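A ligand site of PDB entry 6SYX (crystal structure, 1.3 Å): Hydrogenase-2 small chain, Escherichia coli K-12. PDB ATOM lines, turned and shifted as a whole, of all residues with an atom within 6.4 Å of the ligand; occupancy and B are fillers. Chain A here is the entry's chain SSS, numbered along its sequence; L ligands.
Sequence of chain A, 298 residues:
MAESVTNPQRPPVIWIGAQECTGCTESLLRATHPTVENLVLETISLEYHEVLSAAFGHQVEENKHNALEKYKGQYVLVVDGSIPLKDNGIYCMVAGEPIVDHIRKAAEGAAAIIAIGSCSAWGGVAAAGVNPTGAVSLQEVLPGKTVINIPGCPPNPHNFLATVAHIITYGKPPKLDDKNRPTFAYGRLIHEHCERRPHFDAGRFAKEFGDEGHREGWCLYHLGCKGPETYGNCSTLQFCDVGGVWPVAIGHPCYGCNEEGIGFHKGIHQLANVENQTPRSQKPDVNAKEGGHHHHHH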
ATOM      1  N   ILE A 190      24.042 -36.502  23.708  1.00  0.00           N
ATOM      2  CA  ILE A 190      24.123 -35.037  23.534  1.00  0.00           C
ATOM      3  C   ILE A 190      23.836 -34.356  24.869  1.00  0.00           C
ATOM      4  O   ILE A 190      24.558 -33.422  25.263  1.00  0.00           O
ATOM      5  CB  ILE A 190      23.220 -34.579  22.358  1.00  0.00           C
ATOM      6  CG1 ILE A 190      23.770 -35.086  21.031  1.00  0.00           C
ATOM      7  CG2 ILE A 190      22.993 -33.076  22.354  1.00  0.00           C
ATOM      8  CD1 ILE A 190      22.853 -34.898  19.830  1.00  0.00           C
ATOM      9  N   HIS A 191      22.810 -34.807  25.614  1.00  0.00           N
ATOM     10  CA  HIS A 191      22.423 -34.208  26.935  1.00  0.00           C
ATOM     11  C   HIS A 191      23.503 -34.395  28.009  1.00  0.00           C
ATOM     12  O   HIS A 191      23.468 -33.635  29.004  1.00  0.00           O
ATOM     13  CB  HIS A 191      21.095 -34.836  27.393  1.00  0.00           C
ATOM     14  CG  HIS A 191      20.490 -34.351  28.662  1.00  0.00           C
ATOM     15  ND1 HIS A 191      19.794 -33.172  28.794  1.00  0.00           N
ATOM     16  CD2 HIS A 191      20.390 -34.977  29.880  1.00  0.00           C
ATOM     17  CE1 HIS A 191      19.329 -33.103  30.041  1.00  0.00           C
ATOM     18  NE2 HIS A 191      19.671 -34.172  30.710  1.00  0.00           N
ATOM     19  N   GLU A 192      24.393 -35.378  27.852  1.00  0.00           N
ATOM     20  CA  GLU A 192      25.515 -35.547  28.807  1.00  0.00           C
ATOM     21  C   GLU A 192      26.752 -34.722  28.375  1.00  0.00           C
ATOM     22  O   GLU A 192      27.829 -34.834  29.036  1.00  0.00           O
ATOM     23  CB  GLU A 192      25.809 -37.017  29.010  1.00  0.00           C
ATOM     24  CG  GLU A 192      24.667 -37.770  29.728  1.00  0.00           C
ATOM     25  CD  GLU A 192      24.317 -37.229  31.108  1.00  0.00           C
ATOM     26  OE1 GLU A 192      23.139 -36.890  31.374  1.00  0.00           O
ATOM     27  OE2 GLU A 192      25.249 -37.055  31.919  1.00  0.00           O
ATOM     28  N   CYS A 194      25.925 -31.066  26.940  1.00  0.00           N
ATOM     29  CA  CYS A 194      25.191 -29.925  26.366  1.00  0.00           C
ATOM     30  C   CYS A 194      25.367 -28.688  27.251  1.00  0.00           C
ATOM     31  O   CYS A 194      25.126 -28.770  28.502  1.00  0.00           O
ATOM     32  CB  CYS A 194      23.694 -30.243  26.266  1.00  0.00           C
ATOM     33  SG  CYS A 194      22.707 -28.859  25.612  1.00  0.00           S
ATOM     34  N   GLU A 195      25.670 -27.543  26.655  1.00  0.00           N
ATOM     35  CA  GLU A 195      25.912 -26.282  27.377  1.00  0.00           C
ATOM     36  C   GLU A 195      24.644 -25.697  27.998  1.00  0.00           C
ATOM     37  O   GLU A 195      24.769 -24.747  28.828  1.00  0.00           O
ATOM     38  CB  GLU A 195      26.617 -25.284  26.464  1.00  0.00           C
ATOM     39  CG  GLU A 195      25.800 -24.744  25.267  1.00  0.00           C
ATOM     40  CD  GLU A 195      25.737 -25.541  23.963  1.00  0.00           C
ATOM     41  OE1 GLU A 195      26.108 -26.748  23.958  1.00  0.00           O
ATOM     42  OE2 GLU A 195      25.269 -24.894  22.922  1.00  0.00           O
ATOM     43  N   ARG A 196      23.437 -26.223  27.674  1.00  0.00           N
ATOM     44  CA  ARG A 196      22.189 -25.749  28.318  1.00  0.00           C
ATOM     45  C   ARG A 196      21.843 -26.628  29.513  1.00  0.00           C
ATOM     46  O   ARG A 196      20.806 -26.330  30.192  1.00  0.00           O
ATOM     47  CB  ARG A 196      21.025 -25.602  27.325  1.00  0.00           C
ATOM     48  CG  ARG A 196      21.413 -24.727  26.141  1.00  0.00           C
ATOM     49  CD  ARG A 196      20.263 -24.229  25.301  1.00  0.00           C
ATOM     50  NE  ARG A 196      20.742 -23.262  24.309  1.00  0.00           N
ATOM     51  CZ  ARG A 196      19.980 -22.458  23.618  1.00  0.00           C
ATOM     52  NH1 ARG A 196      18.645 -22.443  23.768  1.00  0.00           N
ATOM     53  NH2 ARG A 196      20.555 -21.615  22.778  1.00  0.00           N
ATOM     54  N   ARG A 197      22.654 -27.609  29.882  1.00  0.00           N
ATOM     55  CA  ARG A 197      22.339 -28.462  31.058  1.00  0.00           C
ATOM     56  C   ARG A 197      22.172 -27.634  32.335  1.00  0.00           C
ATOM     57  O   ARG A 197      21.303 -27.995  33.145  1.00  0.00           O
ATOM     58  CB  ARG A 197      23.419 -29.525  31.250  1.00  0.00           C
ATOM     59  CG  ARG A 197      23.186 -30.467  32.435  1.00  0.00           C
ATOM     60  CD  ARG A 197      21.898 -31.298  32.309  1.00  0.00           C
ATOM     61  NE  ARG A 197      21.848 -32.287  33.421  1.00  0.00           N
ATOM     62  CZ  ARG A 197      22.378 -33.508  33.369  1.00  0.00           C
ATOM     63  NH1 ARG A 197      22.799 -34.023  32.237  1.00  0.00           N
ATOM     64  NH2 ARG A 197      22.486 -34.253  34.468  1.00  0.00           N
ATOM     65  N   PRO A 198      22.927 -26.536  32.612  1.00  0.00           N
ATOM     66  CA  PRO A 198      22.619 -25.759  33.840  1.00  0.00           C
ATOM     67  C   PRO A 198      21.154 -25.285  33.887  1.00  0.00           C
ATOM     68  O   PRO A 198      20.589 -25.158  35.023  1.00  0.00           O
ATOM     69  CB  PRO A 198      23.582 -24.567  33.744  1.00  0.00           C
ATOM     70  CG  PRO A 198      24.734 -25.098  32.885  1.00  0.00           C
ATOM     71  CD  PRO A 198      24.047 -25.969  31.842  1.00  0.00           C
ATOM     72  N   PHE A 200      18.461 -26.705  32.377  1.00  0.00           N
ATOM     73  CA  PHE A 200      17.662 -27.926  32.677  1.00  0.00           C
ATOM     74  C   PHE A 200      17.672 -28.119  34.210  1.00  0.00           C
ATOM     75  O   PHE A 200      16.582 -28.356  34.827  1.00  0.00           O
ATOM     76  CB  PHE A 200      18.261 -29.123  31.927  1.00  0.00           C
ATOM     77  CG  PHE A 200      17.561 -30.432  32.170  1.00  0.00           C
ATOM     78  CD1 PHE A 200      17.958 -31.266  33.191  1.00  0.00           C
ATOM     79  CD2 PHE A 200      16.597 -30.918  31.291  1.00  0.00           C
ATOM     80  CE1 PHE A 200      17.361 -32.493  33.397  1.00  0.00           C
ATOM     81  CE2 PHE A 200      15.978 -32.149  31.521  1.00  0.00           C
ATOM     82  CZ  PHE A 200      16.381 -32.966  32.553  1.00  0.00           C
ATOM     83  N   PHE A 205      13.282 -23.169  31.428  1.00  0.00           N
ATOM     84  CA  PHE A 205      12.822 -23.797  30.159  1.00  0.00           C
ATOM     85  C   PHE A 205      12.145 -22.801  29.245  1.00  0.00           C
ATOM     86  O   PHE A 205      11.275 -22.039  29.691  1.00  0.00           O
ATOM     87  CB  PHE A 205      11.866 -24.953  30.429  1.00  0.00           C
ATOM     88  CG  PHE A 205      12.388 -26.090  31.268  1.00  0.00           C
ATOM     89  CD1 PHE A 205      13.399 -26.932  30.783  1.00  0.00           C
ATOM     90  CD2 PHE A 205      11.890 -26.368  32.556  1.00  0.00           C
ATOM     91  CE1 PHE A 205      13.861 -28.020  31.480  1.00  0.00           C
ATOM     92  CE2 PHE A 205      12.335 -27.470  33.248  1.00  0.00           C
ATOM     93  CZ  PHE A 205      13.348 -28.271  32.759  1.00  0.00           C
ATOM     94  N   TRP A 218      17.622 -20.498  27.138  1.00  0.00           N
ATOM     95  CA  TRP A 218      17.297 -21.532  28.132  1.00  0.00           C
ATOM     96  C   TRP A 218      17.158 -22.927  27.500  1.00  0.00           C
ATOM     97  O   TRP A 218      17.160 -23.102  26.255  1.00  0.00           O
ATOM     98  CB  TRP A 218      16.067 -21.117  28.950  1.00  0.00           C
ATOM     99  CG  TRP A 218      16.267 -20.011  29.953  1.00  0.00           C
ATOM    100  CD1 TRP A 218      17.407 -19.284  30.192  1.00  0.00           C
ATOM    101  CD2 TRP A 218      15.251 -19.433  30.819  1.00  0.00           C
ATOM    102  NE1 TRP A 218      17.164 -18.308  31.148  1.00  0.00           N
ATOM    103  CE2 TRP A 218      15.867 -18.397  31.539  1.00  0.00           C
ATOM    104  CE3 TRP A 218      13.911 -19.754  31.085  1.00  0.00           C
ATOM    105  CZ2 TRP A 218      15.182 -17.700  32.568  1.00  0.00           C
ATOM    106  CZ3 TRP A 218      13.238 -19.036  32.054  1.00  0.00           C
ATOM    107  CH2 TRP A 218      13.853 -18.014  32.755  1.00  0.00           C
ATOM    108  N   CYS A 219      17.035 -23.957  28.329  1.00  0.00           N
ATOM    109  CA  CYS A 219      16.947 -25.368  27.886  1.00  0.00           C
ATOM    110  C   CYS A 219      15.676 -25.600  27.064  1.00  0.00           C
ATOM    111  O   CYS A 219      14.637 -24.981  27.322  1.00  0.00           O
ATOM    112  CB  CYS A 219      17.027 -26.327  29.056  1.00  0.00           C
ATOM    113  SG  CYS A 219      16.570 -28.060  28.749  1.00  0.00           S
ATOM    114  N   LEU A 220      15.790 -26.414  26.004  1.00  0.00           N
ATOM    115  CA  LEU A 220      14.718 -26.707  25.023  1.00  0.00           C
ATOM    116  C   LEU A 220      13.960 -28.023  25.328  1.00  0.00           C
ATOM    117  O   LEU A 220      13.164 -28.514  24.450  1.00  0.00           O
ATOM    118  CB  LEU A 220      15.307 -26.642  23.612  1.00  0.00           C
ATOM    119  CG  LEU A 220      16.074 -25.358  23.259  1.00  0.00           C
ATOM    120  CD1 LEU A 220      16.441 -25.399  21.761  1.00  0.00           C
ATOM    121  CD2 LEU A 220      15.279 -24.114  23.564  1.00  0.00           C
ATOM    122  N   TYR A 221      14.159 -28.640  26.508  1.00  0.00           N
ATOM    123  CA  TYR A 221      13.527 -29.956  26.853  1.00  0.00           C
ATOM    124  C   TYR A 221      11.994 -29.907  26.602  1.00  0.00           C
ATOM    125  O   TYR A 221      11.419 -30.868  26.007  1.00  0.00           O
ATOM    126  CB  TYR A 221      13.811 -30.354  28.320  1.00  0.00           C
ATOM    127  CG  TYR A 221      13.145 -31.671  28.682  1.00  0.00           C
ATOM    128  CD1 TYR A 221      13.616 -32.874  28.206  1.00  0.00           C
ATOM    129  CD2 TYR A 221      11.958 -31.713  29.396  1.00  0.00           C
ATOM    130  CE1 TYR A 221      13.017 -34.101  28.463  1.00  0.00           C
ATOM    131  CE2 TYR A 221      11.299 -32.925  29.634  1.00  0.00           C
ATOM    132  CZ  TYR A 221      11.795 -34.108  29.133  1.00  0.00           C
ATOM    133  OH  TYR A 221      11.121 -35.307  29.343  1.00  0.00           O
ATOM    134  N   HIS A 222      11.322 -28.878  27.123  1.00  0.00           N
ATOM    135  CA  HIS A 222       9.834 -28.803  27.002  1.00  0.00           C
ATOM    136  C   HIS A 222       9.374 -28.377  25.617  1.00  0.00           C
ATOM    137  O   HIS A 222       8.139 -28.356  25.425  1.00  0.00           O
ATOM    138  CB  HIS A 222       9.246 -27.947  28.130  1.00  0.00           C
ATOM    139  CG  HIS A 222       9.184 -28.708  29.421  1.00  0.00           C
ATOM    140  ND1 HIS A 222       8.230 -29.671  29.645  1.00  0.00           N
ATOM    141  CD2 HIS A 222       9.963 -28.649  30.538  1.00  0.00           C
ATOM    142  CE1 HIS A 222       8.461 -30.235  30.832  1.00  0.00           C
ATOM    143  NE2 HIS A 222       9.511 -29.623  31.430  1.00  0.00           N
ATOM    144  N   CYS A 225      13.128 -31.473  22.962  1.00  0.00           N
ATOM    145  CA  CYS A 225      14.544 -31.812  22.706  1.00  0.00           C
ATOM    146  C   CYS A 225      14.805 -33.295  22.920  1.00  0.00           C
ATOM    147  O   CYS A 225      14.518 -33.832  24.037  1.00  0.00           O
ATOM    148  CB  CYS A 225      15.465 -30.936  23.554  1.00  0.00           C
ATOM    149  SG  CYS A 225      17.228 -31.166  23.084  1.00  0.00           S
ATOM    150  N   LYS A 226      15.418 -33.971  21.959  1.00  0.00           N
ATOM    151  CA  LYS A 226      15.747 -35.415  22.043  1.00  0.00           C
ATOM    152  C   LYS A 226      17.213 -35.643  22.471  1.00  0.00           C
ATOM    153  O   LYS A 226      17.669 -36.819  22.472  1.00  0.00           O
ATOM    154  CB  LYS A 226      15.418 -36.132  20.737  1.00  0.00           C
ATOM    155  CG  LYS A 226      13.969 -35.970  20.249  1.00  0.00           C
ATOM    156  CD  LYS A 226      12.899 -36.346  21.284  1.00  0.00           C
ATOM    157  CE  LYS A 226      11.479 -36.381  20.783  1.00  0.00           C
ATOM    158  NZ  LYS A 226      11.089 -35.119  20.100  1.00  0.00           N
ATOM    159  N   GLY A 227      17.905 -34.579  22.871  1.00  0.00           N
ATOM    160  CA  GLY A 227      19.311 -34.750  23.391  1.00  0.00           C
ATOM    161  C   GLY A 227      19.405 -35.841  24.494  1.00  0.00           C
ATOM    162  O   GLY A 227      20.405 -36.600  24.500  1.00  0.00           O
ATOM    163  N   PRO A 228      18.399 -36.000  25.418  1.00  0.00           N
ATOM    164  CA  PRO A 228      18.497 -37.038  26.458  1.00  0.00           C
ATOM    165  C   PRO A 228      18.535 -38.478  25.966  1.00  0.00           C
ATOM    166  O   PRO A 228      18.950 -39.394  26.729  1.00  0.00           O
ATOM    167  CB  PRO A 228      17.294 -36.753  27.358  1.00  0.00           C
ATOM    168  CG  PRO A 228      17.021 -35.292  27.189  1.00  0.00           C
ATOM    169  CD  PRO A 228      17.312 -35.046  25.692  1.00  0.00           C
ATOM    170  N   TRP A 246      24.789 -25.303  15.903  1.00  0.00           N
ATOM    171  CA  TRP A 246      24.083 -26.611  15.926  1.00  0.00           C
ATOM    172  C   TRP A 246      22.617 -26.300  16.188  1.00  0.00           C
ATOM    173  O   TRP A 246      22.291 -25.136  16.570  1.00  0.00           O
ATOM    174  CB  TRP A 246      24.721 -27.611  16.929  1.00  0.00           C
ATOM    175  CG  TRP A 246      24.587 -27.343  18.403  1.00  0.00           C
ATOM    176  CD1 TRP A 246      25.193 -26.364  19.180  1.00  0.00           C
ATOM    177  CD2 TRP A 246      23.869 -28.196  19.339  1.00  0.00           C
ATOM    178  NE1 TRP A 246      24.927 -26.581  20.515  1.00  0.00           N
ATOM    179  CE2 TRP A 246      24.095 -27.678  20.650  1.00  0.00           C
ATOM    180  CE3 TRP A 246      23.120 -29.375  19.218  1.00  0.00           C
ATOM    181  CZ2 TRP A 246      23.591 -28.301  21.805  1.00  0.00           C
ATOM    182  CZ3 TRP A 246      22.594 -29.964  20.351  1.00  0.00           C
ATOM    183  CH2 TRP A 246      22.876 -29.454  21.629  1.00  0.00           C
ATOM    184  N   VAL A 248      20.304 -26.745  18.576  1.00  0.00           N
ATOM    185  CA  VAL A 248      19.914 -26.186  19.915  1.00  0.00           C
ATOM    186  C   VAL A 248      20.494 -24.783  20.050  1.00  0.00           C
ATOM    187  O   VAL A 248      19.776 -23.846  20.498  1.00  0.00           O
ATOM    188  CB  VAL A 248      20.360 -27.120  21.034  1.00  0.00           C
ATOM    189  CG1 VAL A 248      20.351 -26.406  22.380  1.00  0.00           C
ATOM    190  CG2 VAL A 248      19.466 -28.374  21.066  1.00  0.00           C
ATOM    191  N   PRO A 253      14.893 -27.528  19.238  1.00  0.00           N
ATOM    192  CA  PRO A 253      15.286 -28.789  19.884  1.00  0.00           C
ATOM    193  C   PRO A 253      15.982 -29.770  18.930  1.00  0.00           C
ATOM    194  O   PRO A 253      15.715 -29.790  17.706  1.00  0.00           O
ATOM    195  CB  PRO A 253      13.921 -29.356  20.360  1.00  0.00           C
ATOM    196  CG  PRO A 253      12.894 -28.629  19.504  1.00  0.00           C
ATOM    197  CD  PRO A 253      13.464 -27.244  19.293  1.00  0.00           C
ATOM    198  N   CYS A 254      16.858 -30.616  19.481  1.00  0.00           N
ATOM    199  CA  CYS A 254      17.280 -31.827  18.753  1.00  0.00           C
ATOM    200  C   CYS A 254      16.045 -32.697  18.464  1.00  0.00           C
ATOM    201  O   CYS A 254      15.144 -32.837  19.335  1.00  0.00           O
ATOM    202  CB  CYS A 254      18.331 -32.599  19.590  1.00  0.00           C
ATOM    203  SG  CYS A 254      18.809 -34.264  18.985  1.00  0.00           S
HETATM  204 FE1  LIG L   1      18.165 -29.159  27.473  1.00  0.00          FE
HETATM  205 FE2  LIG L   1      18.296 -30.603  25.073  1.00  0.00          FE
HETATM  206 FE3  LIG L   1      19.382 -31.626  27.418  1.00  0.00          FE
HETATM  207 FE4  LIG L   1      20.576 -29.532  26.155  1.00  0.00          FE
HETATM  208  S1  LIG L   1      20.325 -31.731  25.319  1.00  0.00           S
HETATM  209  S2  LIG L   1      20.191 -29.676  28.434  1.00  0.00           S
HETATM  210  S3  LIG L   1      18.744 -28.323  25.396  1.00  0.00           S
HETATM  211  S4  LIG L   1      17.153 -31.246  26.992  1.00  0.00           S
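Residues that only touch the ligand: Arg 196 (3.6 Å), Tyr 221 (3.7 Å), Gly 227 (3.7 Å) and Val 248 (3.9 Å). Within 4 Å of the ligand: His 191, Cys 194, Arg 196, Arg 197, Cys 219, Leu 220, Tyr 221, Cys 225, Gly 227 and Val 248. The nearest printed residue that does not touch the ligand is Pro 228 (4.02 Å).
The backbone NH of His 191 sits at hydrogen-bond distance from the backbone carbonyl oxygen of Gly 227 (3.2 Å). The side-chain sulfur (SG) of Cys 219 sits close to the backbone NH (N) of Tyr 221, at 3.3 Å. The backbone carbonyl oxygen (O) of Leu 220 is in hydrogen-bond range of the backbone NH (N) of Cys 225, 3.3 Å away. SG of Cys 225 lies close to N of Gly 227, at 3.5 Å. SG of Cys 225 sits close to N of Cys 254 (3.7 Å). NH1 of Arg 197 is in salt-bridge range of OE1 of Glu 192 (3.0 Å). NH2 of Arg 196 sits at hydrogen-bond distance from O of Val 248, 3.3 Å away. NH1 of Arg 196 lies within hydrogen-bond range of O of Trp 218.
ND1 of His 191 is bound to FE3 of the ligand (2.1 Å). The side-chain sulfur (SG) of Cys 194 is bound to an iron atom (FE4) of the ligand (2.3 Å). FE1 of the ligand is bound by SG of Cys 219. FE2 of the ligand is bound by SG of Cys 225. N of Arg 197 lies close to S2 of the ligand, at 3.5 Å. S3 of the ligand lies close to N of Leu 220, at 3.6 Å.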
